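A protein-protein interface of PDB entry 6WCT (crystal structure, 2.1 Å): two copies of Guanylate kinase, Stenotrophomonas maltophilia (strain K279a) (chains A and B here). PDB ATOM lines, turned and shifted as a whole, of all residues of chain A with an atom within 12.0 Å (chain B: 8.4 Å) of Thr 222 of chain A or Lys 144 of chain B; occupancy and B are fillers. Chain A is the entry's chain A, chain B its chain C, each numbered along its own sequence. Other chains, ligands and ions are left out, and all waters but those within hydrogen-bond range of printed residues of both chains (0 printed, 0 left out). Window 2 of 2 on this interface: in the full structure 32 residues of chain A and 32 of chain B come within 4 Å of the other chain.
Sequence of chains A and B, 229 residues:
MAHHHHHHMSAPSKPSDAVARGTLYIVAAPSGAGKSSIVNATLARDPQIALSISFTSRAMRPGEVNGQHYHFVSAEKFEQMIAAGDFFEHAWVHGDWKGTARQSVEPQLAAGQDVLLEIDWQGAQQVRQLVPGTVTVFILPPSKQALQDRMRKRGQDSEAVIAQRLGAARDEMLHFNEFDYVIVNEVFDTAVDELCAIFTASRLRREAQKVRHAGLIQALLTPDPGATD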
ATOM      1  N   HIS A 213      19.843 -37.782  14.077  1.00  0.00           N
ATOM      2  CA  HIS A 213      20.119 -36.512  14.743  1.00  0.00           C
ATOM      3  C   HIS A 213      20.046 -35.332  13.779  1.00  0.00           C
ATOM      4  O   HIS A 213      20.769 -34.344  13.945  1.00  0.00           O
ATOM      5  CB  HIS A 213      21.484 -36.546  15.433  1.00  0.00           C
ATOM      6  CG  HIS A 213      21.596 -37.580  16.509  1.00  0.00           C
ATOM      7  ND1 HIS A 213      22.106 -38.841  16.282  1.00  0.00           N
ATOM      8  CD2 HIS A 213      21.262 -37.540  17.821  1.00  0.00           C
ATOM      9  CE1 HIS A 213      22.088 -39.531  17.407  1.00  0.00           C
ATOM     10  NE2 HIS A 213      21.576 -38.766  18.356  1.00  0.00           N
ATOM     11  N   ALA A 214      19.186 -35.429  12.761  1.00  0.00           N
ATOM     12  CA  ALA A 214      19.087 -34.373  11.755  1.00  0.00           C
ATOM     13  C   ALA A 214      18.840 -33.013  12.395  1.00  0.00           C
ATOM     14  O   ALA A 214      19.485 -32.020  12.042  1.00  0.00           O
ATOM     15  CB  ALA A 214      17.980 -34.700  10.752  1.00  0.00           C
ATOM     16  N   GLY A 215      17.901 -32.952  13.340  1.00  0.00           N
ATOM     17  CA  GLY A 215      17.583 -31.679  13.966  1.00  0.00           C
ATOM     18  C   GLY A 215      18.745 -31.120  14.761  1.00  0.00           C
ATOM     19  O   GLY A 215      19.041 -29.925  14.690  1.00  0.00           O
ATOM     20  N   LEU A 216      19.419 -31.980  15.532  1.00  0.00           N
ATOM     21  CA  LEU A 216      20.598 -31.536  16.271  1.00  0.00           C
ATOM     22  C   LEU A 216      21.674 -31.009  15.332  1.00  0.00           C
ATOM     23  O   LEU A 216      22.259 -29.946  15.579  1.00  0.00           O
ATOM     24  CB  LEU A 216      21.149 -32.681  17.116  1.00  0.00           C
ATOM     25  CG  LEU A 216      22.487 -32.373  17.780  1.00  0.00           C
ATOM     26  CD1 LEU A 216      22.323 -31.252  18.780  1.00  0.00           C
ATOM     27  CD2 LEU A 216      23.030 -33.614  18.449  1.00  0.00           C
ATOM     28  N   ILE A 217      21.929 -31.727  14.234  1.00  0.00           N
ATOM     29  CA  ILE A 217      22.972 -31.314  13.295  1.00  0.00           C
ATOM     30  C   ILE A 217      22.615 -29.969  12.676  1.00  0.00           C
ATOM     31  O   ILE A 217      23.474 -29.091  12.524  1.00  0.00           O
ATOM     32  CB  ILE A 217      23.189 -32.393  12.218  1.00  0.00           C
ATOM     33  CG1 ILE A 217      23.782 -33.655  12.838  1.00  0.00           C
ATOM     34  CG2 ILE A 217      24.118 -31.879  11.127  1.00  0.00           C
ATOM     35  CD1 ILE A 217      23.719 -34.877  11.921  1.00  0.00           C
ATOM     36  N   GLN A 218      21.343 -29.788  12.312  1.00  0.00           N
ATOM     37  CA  GLN A 218      20.908 -28.518  11.742  1.00  0.00           C
ATOM     38  C   GLN A 218      21.159 -27.366  12.712  1.00  0.00           C
ATOM     39  O   GLN A 218      21.602 -26.286  12.303  1.00  0.00           O
ATOM     40  CB  GLN A 218      19.429 -28.598  11.362  1.00  0.00           C
ATOM     41  N   ALA A 219      20.887 -27.580  14.002  1.00  0.00           N
ATOM     42  CA  ALA A 219      21.133 -26.549  15.009  1.00  0.00           C
ATOM     43  C   ALA A 219      22.623 -26.236  15.156  1.00  0.00           C
ATOM     44  O   ALA A 219      23.015 -25.065  15.234  1.00  0.00           O
ATOM     45  CB  ALA A 219      20.541 -26.986  16.350  1.00  0.00           C
ATOM     46  N   LEU A 220      23.468 -27.271  15.220  1.00  0.00           N
ATOM     47  CA  LEU A 220      24.895 -27.056  15.459  1.00  0.00           C
ATOM     48  C   LEU A 220      25.586 -26.358  14.295  1.00  0.00           C
ATOM     49  O   LEU A 220      26.523 -25.581  14.510  1.00  0.00           O
ATOM     50  CB  LEU A 220      25.590 -28.387  15.754  1.00  0.00           C
ATOM     51  CG  LEU A 220      25.278 -29.056  17.091  1.00  0.00           C
ATOM     52  CD1 LEU A 220      25.969 -30.408  17.172  1.00  0.00           C
ATOM     53  CD2 LEU A 220      25.729 -28.162  18.236  1.00  0.00           C
ATOM     54  N   LEU A 221      25.150 -26.614  13.067  1.00  0.00           N
ATOM     55  CA  LEU A 221      25.821 -26.070  11.894  1.00  0.00           C
ATOM     56  C   LEU A 221      25.216 -24.752  11.438  1.00  0.00           C
ATOM     57  O   LEU A 221      25.712 -24.145  10.483  1.00  0.00           O
ATOM     58  CB  LEU A 221      25.809 -27.091  10.750  1.00  0.00           C
ATOM     59  CG  LEU A 221      26.995 -28.070  10.707  1.00  0.00           C
ATOM     60  CD1 LEU A 221      27.366 -28.621  12.082  1.00  0.00           C
ATOM     61  CD2 LEU A 221      26.727 -29.213   9.735  1.00  0.00           C
ATOM     62  N   THR A 222      24.171 -24.313  12.078  1.00  0.00           N
ATOM     63  CA  THR A 222      23.593 -23.024  11.748  1.00  0.00           C
ATOM     64  C   THR A 222      24.414 -21.917  12.411  1.00  0.00           C
ATOM     65  O   THR A 222      24.955 -22.114  13.504  1.00  0.00           O
ATOM     66  CB  THR A 222      22.120 -22.962  12.185  1.00  0.00           C
ATOM     67  OG1 THR A 222      21.401 -22.093  11.305  1.00  0.00           O
ATOM     68  CG2 THR A 222      21.968 -22.468  13.620  1.00  0.00           C
ATOM     69  N   PRO A 223      24.608 -20.778  11.733  1.00  0.00           N
ATOM     70  CA  PRO A 223      25.380 -19.681  12.328  1.00  0.00           C
ATOM     71  C   PRO A 223      24.551 -18.828  13.286  1.00  0.00           C
ATOM     72  O   PRO A 223      25.071 -17.847  13.815  1.00  0.00           O
ATOM     73  CB  PRO A 223      25.812 -18.862  11.113  1.00  0.00           C
ATOM     74  CG  PRO A 223      24.735 -19.098  10.104  1.00  0.00           C
ATOM     75  CD  PRO A 223      24.140 -20.459  10.374  1.00  0.00           C
ATOM     76  N   GLY B  32      34.793 -28.245  23.445  1.00  0.00           N
ATOM     77  CA  GLY B  32      33.565 -28.170  24.208  1.00  0.00           C
ATOM     78  C   GLY B  32      32.588 -29.292  23.959  1.00  0.00           C
ATOM     79  O   GLY B  32      31.468 -29.242  24.487  1.00  0.00           O
ATOM     80  N   PRO B 141      28.578 -32.279  20.404  1.00  0.00           N
ATOM     81  CA  PRO B 141      27.917 -31.981  21.684  1.00  0.00           C
ATOM     82  C   PRO B 141      26.431 -32.277  21.595  1.00  0.00           C
ATOM     83  O   PRO B 141      25.851 -32.239  20.501  1.00  0.00           O
ATOM     84  CB  PRO B 141      28.178 -30.483  21.875  1.00  0.00           C
ATOM     85  CG  PRO B 141      28.322 -29.965  20.476  1.00  0.00           C
ATOM     86  CD  PRO B 141      29.026 -31.052  19.716  1.00  0.00           C
ATOM     87  N   PRO B 142      25.774 -32.551  22.727  1.00  0.00           N
ATOM     88  CA  PRO B 142      24.356 -32.948  22.678  1.00  0.00           C
ATOM     89  C   PRO B 142      23.389 -31.826  22.337  1.00  0.00           C
ATOM     90  O   PRO B 142      22.210 -32.124  22.100  1.00  0.00           O
ATOM     91  CB  PRO B 142      24.097 -33.482  24.088  1.00  0.00           C
ATOM     92  CG  PRO B 142      25.050 -32.732  24.945  1.00  0.00           C
ATOM     93  CD  PRO B 142      26.294 -32.524  24.105  1.00  0.00           C
ATOM     94  N   SER B 143      23.825 -30.569  22.298  1.00  0.00           N
ATOM     95  CA  SER B 143      22.931 -29.471  21.943  1.00  0.00           C
ATOM     96  C   SER B 143      23.755 -28.211  21.759  1.00  0.00           C
ATOM     97  O   SER B 143      24.903 -28.130  22.204  1.00  0.00           O
ATOM     98  CB  SER B 143      21.846 -29.236  23.003  1.00  0.00           C
ATOM     99  OG  SER B 143      22.408 -28.722  24.193  1.00  0.00           O
ATOM    100  N   LYS B 144      23.138 -27.218  21.108  1.00  0.00           N
ATOM    101  CA  LYS B 144      23.804 -25.935  20.918  1.00  0.00           C
ATOM    102  C   LYS B 144      24.058 -25.253  22.254  1.00  0.00           C
ATOM    103  O   LYS B 144      25.108 -24.630  22.453  1.00  0.00           O
ATOM    104  CB  LYS B 144      22.963 -25.042  20.002  1.00  0.00           C
ATOM    105  CG  LYS B 144      23.661 -23.774  19.525  1.00  0.00           C
ATOM    106  CD  LYS B 144      24.738 -24.074  18.490  1.00  0.00           C
ATOM    107  CE  LYS B 144      25.370 -22.794  17.948  1.00  0.00           C
ATOM    108  NZ  LYS B 144      24.423 -21.999  17.123  1.00  0.00           N
ATOM    109  N   GLN B 145      23.114 -25.374  23.192  1.00  0.00           N
ATOM    110  CA  GLN B 145      23.334 -24.830  24.528  1.00  0.00           C
ATOM    111  C   GLN B 145      24.509 -25.518  25.214  1.00  0.00           C
ATOM    112  O   GLN B 145      25.348 -24.855  25.831  1.00  0.00           O
ATOM    113  CB  GLN B 145      22.064 -24.962  25.370  1.00  0.00           C
ATOM    114  N   ALA B 146      24.592 -26.848  25.109  1.00  0.00           N
ATOM    115  CA  ALA B 146      25.680 -27.569  25.763  1.00  0.00           C
ATOM    116  C   ALA B 146      27.040 -27.103  25.257  1.00  0.00           C
ATOM    117  O   ALA B 146      27.986 -26.965  26.040  1.00  0.00           O
ATOM    118  CB  ALA B 146      25.513 -29.071  25.542  1.00  0.00           C
ATOM    119  N   LEU B 147      27.144 -26.821  23.956  1.00  0.00           N
ATOM    120  CA  LEU B 147      28.386 -26.298  23.392  1.00  0.00           C
ATOM    121  C   LEU B 147      28.702 -24.910  23.941  1.00  0.00           C
ATOM    122  O   LEU B 147      29.832 -24.642  24.367  1.00  0.00           O
ATOM    123  CB  LEU B 147      28.296 -26.263  21.867  1.00  0.00           C
ATOM    124  CG  LEU B 147      29.603 -25.920  21.145  1.00  0.00           C
ATOM    125  CD1 LEU B 147      30.683 -26.948  21.473  1.00  0.00           C
ATOM    126  CD2 LEU B 147      29.394 -25.790  19.635  1.00  0.00           C
ATOM    127  N   GLN B 148      27.713 -24.010  23.928  1.00  0.00           N
ATOM    128  CA  GLN B 148      27.930 -22.657  24.437  1.00  0.00           C
ATOM    129  C   GLN B 148      28.322 -22.678  25.911  1.00  0.00           C
ATOM    130  O   GLN B 148      29.229 -21.949  26.329  1.00  0.00           O
ATOM    131  CB  GLN B 148      26.678 -21.803  24.220  1.00  0.00           C
ATOM    132  N   ASP B 149      27.653 -23.515  26.711  1.00  0.00           N
ATOM    133  CA  ASP B 149      27.909 -23.549  28.148  1.00  0.00           C
ATOM    134  C   ASP B 149      29.354 -23.937  28.446  1.00  0.00           C
ATOM    135  O   ASP B 149      30.005 -23.327  29.301  1.00  0.00           O
ATOM    136  CB  ASP B 149      26.942 -24.526  28.824  1.00  0.00           C
ATOM    137  CG  ASP B 149      25.484 -24.102  28.689  1.00  0.00           C
ATOM    138  OD1 ASP B 149      25.226 -22.928  28.347  1.00  0.00           O
ATOM    139  OD2 ASP B 149      24.596 -24.954  28.908  1.00  0.00           O
ATOM    140  N   ARG B 150      29.871 -24.948  27.746  1.00  0.00           N
ATOM    141  CA  ARG B 150      31.228 -25.435  27.977  1.00  0.00           C
ATOM    142  C   ARG B 150      32.292 -24.405  27.612  1.00  0.00           C
ATOM    143  O   ARG B 150      33.418 -24.487  28.117  1.00  0.00           O
ATOM    144  CB  ARG B 150      31.466 -26.734  27.193  1.00  0.00           C
ATOM    145  N   MET B 151      31.962 -23.433  26.767  1.00  0.00           N
ATOM    146  CA  MET B 151      32.944 -22.490  26.246  1.00  0.00           C
ATOM    147  C   MET B 151      33.302 -21.427  27.285  1.00  0.00           C
ATOM    148  O   MET B 151      32.425 -20.841  27.926  1.00  0.00           O
ATOM    149  CB  MET B 151      32.377 -21.795  25.003  1.00  0.00           C
ATOM    150  CG  MET B 151      32.428 -22.588  23.702  1.00  0.00           C
ATOM    151  SD  MET B 151      34.007 -23.230  23.136  1.00  0.00           S
ATOM    152  CE  MET B 151      33.485 -24.052  21.626  1.00  0.00           C
ATOM    153  N   LEU B 166      33.351 -20.238  19.477  1.00  0.00           N
ATOM    154  CA  LEU B 166      32.154 -20.851  18.906  1.00  0.00           C
ATOM    155  C   LEU B 166      32.227 -20.890  17.386  1.00  0.00           C
ATOM    156  O   LEU B 166      31.808 -21.872  16.762  1.00  0.00           O
ATOM    157  CB  LEU B 166      30.892 -20.119  19.367  1.00  0.00           C
ATOM    158  CG  LEU B 166      30.456 -20.432  20.798  1.00  0.00           C
ATOM    159  CD1 LEU B 166      29.222 -19.636  21.199  1.00  0.00           C
ATOM    160  CD2 LEU B 166      30.194 -21.921  20.932  1.00  0.00           C
ATOM    161  N   GLY B 167      32.757 -19.832  16.772  1.00  0.00           N
ATOM    162  CA  GLY B 167      32.896 -19.828  15.327  1.00  0.00           C
ATOM    163  C   GLY B 167      33.844 -20.902  14.842  1.00  0.00           C
ATOM    164  O   GLY B 167      33.590 -21.554  13.826  1.00  0.00           O
ATOM    165  N   ALA B 169      34.327 -23.677  16.394  1.00  0.00           N
ATOM    166  CA  ALA B 169      33.638 -24.944  16.618  1.00  0.00           C
ATOM    167  C   ALA B 169      32.735 -25.301  15.441  1.00  0.00           C
ATOM    168  O   ALA B 169      32.728 -26.448  14.977  1.00  0.00           O
ATOM    169  CB  ALA B 169      32.838 -24.886  17.918  1.00  0.00           C
ATOM    170  N   ARG B 170      31.956 -24.332  14.943  1.00  0.00           N
ATOM    171  CA  ARG B 170      31.063 -24.625  13.824  1.00  0.00           C
ATOM    172  C   ARG B 170      31.853 -24.979  12.572  1.00  0.00           C
ATOM    173  O   ARG B 170      31.485 -25.908  11.840  1.00  0.00           O
ATOM    174  CB  ARG B 170      30.153 -23.433  13.521  1.00  0.00           C
ATOM    175  CG  ARG B 170      29.063 -23.773  12.514  1.00  0.00           C
ATOM    176  CD  ARG B 170      28.274 -22.569  12.064  1.00  0.00           C
ATOM    177  NE  ARG B 170      28.950 -21.901  10.961  1.00  0.00           N
ATOM    178  CZ  ARG B 170      28.720 -22.176   9.680  1.00  0.00           C
ATOM    179  NH1 ARG B 170      27.818 -23.093   9.351  1.00  0.00           N
ATOM    180  NH2 ARG B 170      29.384 -21.533   8.728  1.00  0.00           N
ATOM    181  N   ASP B 171      32.945 -24.251  12.317  1.00  0.00           N
ATOM    182  CA  ASP B 171      33.815 -24.570  11.192  1.00  0.00           C
ATOM    183  C   ASP B 171      34.313 -26.001  11.285  1.00  0.00           C
ATOM    184  O   ASP B 171      34.375 -26.714  10.278  1.00  0.00           O
ATOM    185  CB  ASP B 171      35.000 -23.603  11.144  1.00  0.00           C
ATOM    186  CG  ASP B 171      34.589 -22.181  10.811  1.00  0.00           C
ATOM    187  OD1 ASP B 171      33.678 -21.996   9.970  1.00  0.00           O
ATOM    188  OD2 ASP B 171      35.188 -21.247  11.390  1.00  0.00           O
ATOM    189  N   MET B 173      32.802 -28.521  12.980  1.00  0.00           N
ATOM    190  CA  MET B 173      31.666 -29.436  12.851  1.00  0.00           C
ATOM    191  C   MET B 173      31.132 -29.532  11.428  1.00  0.00           C
ATOM    192  O   MET B 173      30.530 -30.551  11.081  1.00  0.00           O
ATOM    193  CB  MET B 173      30.532 -29.011  13.784  1.00  0.00           C
ATOM    194  CG  MET B 173      30.890 -29.119  15.249  1.00  0.00           C
ATOM    195  SD  MET B 173      29.527 -28.787  16.384  1.00  0.00           S
ATOM    196  CE  MET B 173      29.327 -27.013  16.164  1.00  0.00           C
ATOM    197  N   LEU B 174      31.365 -28.519  10.591  1.00  0.00           N
ATOM    198  CA  LEU B 174      30.923 -28.584   9.202  1.00  0.00           C
ATOM    199  C   LEU B 174      31.529 -29.765   8.455  1.00  0.00           C
ATOM    200  O   LEU B 174      31.015 -30.147   7.398  1.00  0.00           O
ATOM    201  CB  LEU B 174      31.268 -27.282   8.469  1.00  0.00           C
ATOM    202  CG  LEU B 174      30.351 -26.083   8.717  1.00  0.00           C
ATOM    203  CD1 LEU B 174      30.908 -24.799   8.091  1.00  0.00           C
ATOM    204  CD2 LEU B 174      28.950 -26.377   8.198  1.00  0.00           C
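The backbone carbonyl oxygen of Leu 221 of chain A lies within hydrogen-bond range of the guanidinium group of Arg 170 of chain B (2.6 Å).
The side-chain hydroxyl (OG) of Ser 143 of chain B sits at hydrogen-bond distance from the backbone NH (N) of Ala 146 of chain B, at 3.0 Å.
Of the 11 printed residues of chain A, 5 touch a printed residue of chain B. Printed residues of chain A that touch a printed residue of chain B: Leu 216, Ala 219, Leu 220, Leu 221 and Thr 222. Of the 19 printed residues of chain B, 7 touch a printed residue of chain A. Hydrophobic or aromatic side chains of chain B within 4 Å of the printed part of chain A: Pro 141, Met 173 and Leu 174. Among the printed residues, no Asp or Glu carboxylate lies within 4 Å of a Lys or Arg side-chain nitrogen of the other chain.
No position is printed for both chains. Of the 13 pairs that touch across the chains among the printed residues, none has its exchanged pair printed and touching as well.
Of chain B, only Lys 144 (3.7 Å) and Arg 170 (3.6 Å) come within 4 Å of Thr 222 of chain A. Of the printed residues of chain A, Lys 144 of chain B touches Ala 219, Leu 220 and Thr 222. No residue of chain B comes within 4 Å of Pro 223 of chain A. Pro 141 of chain B touches just these residues of chain A: Leu 216 and Leu 220. Of chain A, only Leu 216 (3.4 Å) comes within 4 Å of Pro 142 of chain B. Of chain A, only Leu 216 (3.7 Å) comes within 4 Å of Ser 143 of chain B. No residue of chain A comes within 4 Å of Gln 145 of chain B. No residue of chain A comes within 4 Å of Leu 147 of chain B. No residue of chain A comes within 4 Å of Gln 148 of chain B. Of the printed residues of chain A, Arg 170 of chain B touches Leu 220 (3.7 Å), Leu 221 (2.6 Å) and Thr 222 (3.6 Å). Of the printed residues of chain B, Leu 216 of chain A touches Pro 141, Pro 142 and Ser 143. Printed residues of chain B within 4 Å of Leu 220 of chain A: Pro 141 (3.8 Å), Lys 144 (3.98 Å), Arg 170 (3.7 Å) and Met 173 (3.6 Å). Of the printed residues of chain B, Ala 219 of chain A touches Lys 144. Of the printed residues of chain B, Leu 221 of chain A touches Arg 170 (2.6 Å), Met 173 (3.6 Å) and Leu 174 (3.6 Å). Printed residues of chain A within 4 Å of Met 173 of chain B: Leu 220 (3.6 Å) and Leu 221 (3.6 Å). Gly 215 of chain A touches none of the printed residues of chain B. Asp 171 of chain B touches none of the printed residues of chain A. The nearest residue of chain B that does not touch Thr 222 of chain A is Leu 174 of chain B (6.5 Å).
Pro 142 of chain B touches Leu 216 of chain A (O to CD1, 3.4 Å). CA of Ser 143 of chain B touches CD1 of Leu 216 of chain A, 3.7 Å away. Lys 144 of chain B touches Ala 219 of chain A (CD to O, 3.8 Å). Leu 220 of chain A touches Pro 141 of chain B. Leu 220 of chain A touches Lys 144 of chain B (CD2 to N, 3.98 Å). Leu 220 of chain A touches Arg 170 of chain B. Met 173 of chain B touches Leu 220 of chain A. CD1 of Leu 221 of chain A touches CB of Met 173 of chain B, 3.6 Å away. Thr 222 of chain A touches Lys 144 of chain B (O to NZ, 3.7 Å). O of Thr 222 of chain A touches CD of Arg 170 of chain B, at 3.6 Å.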
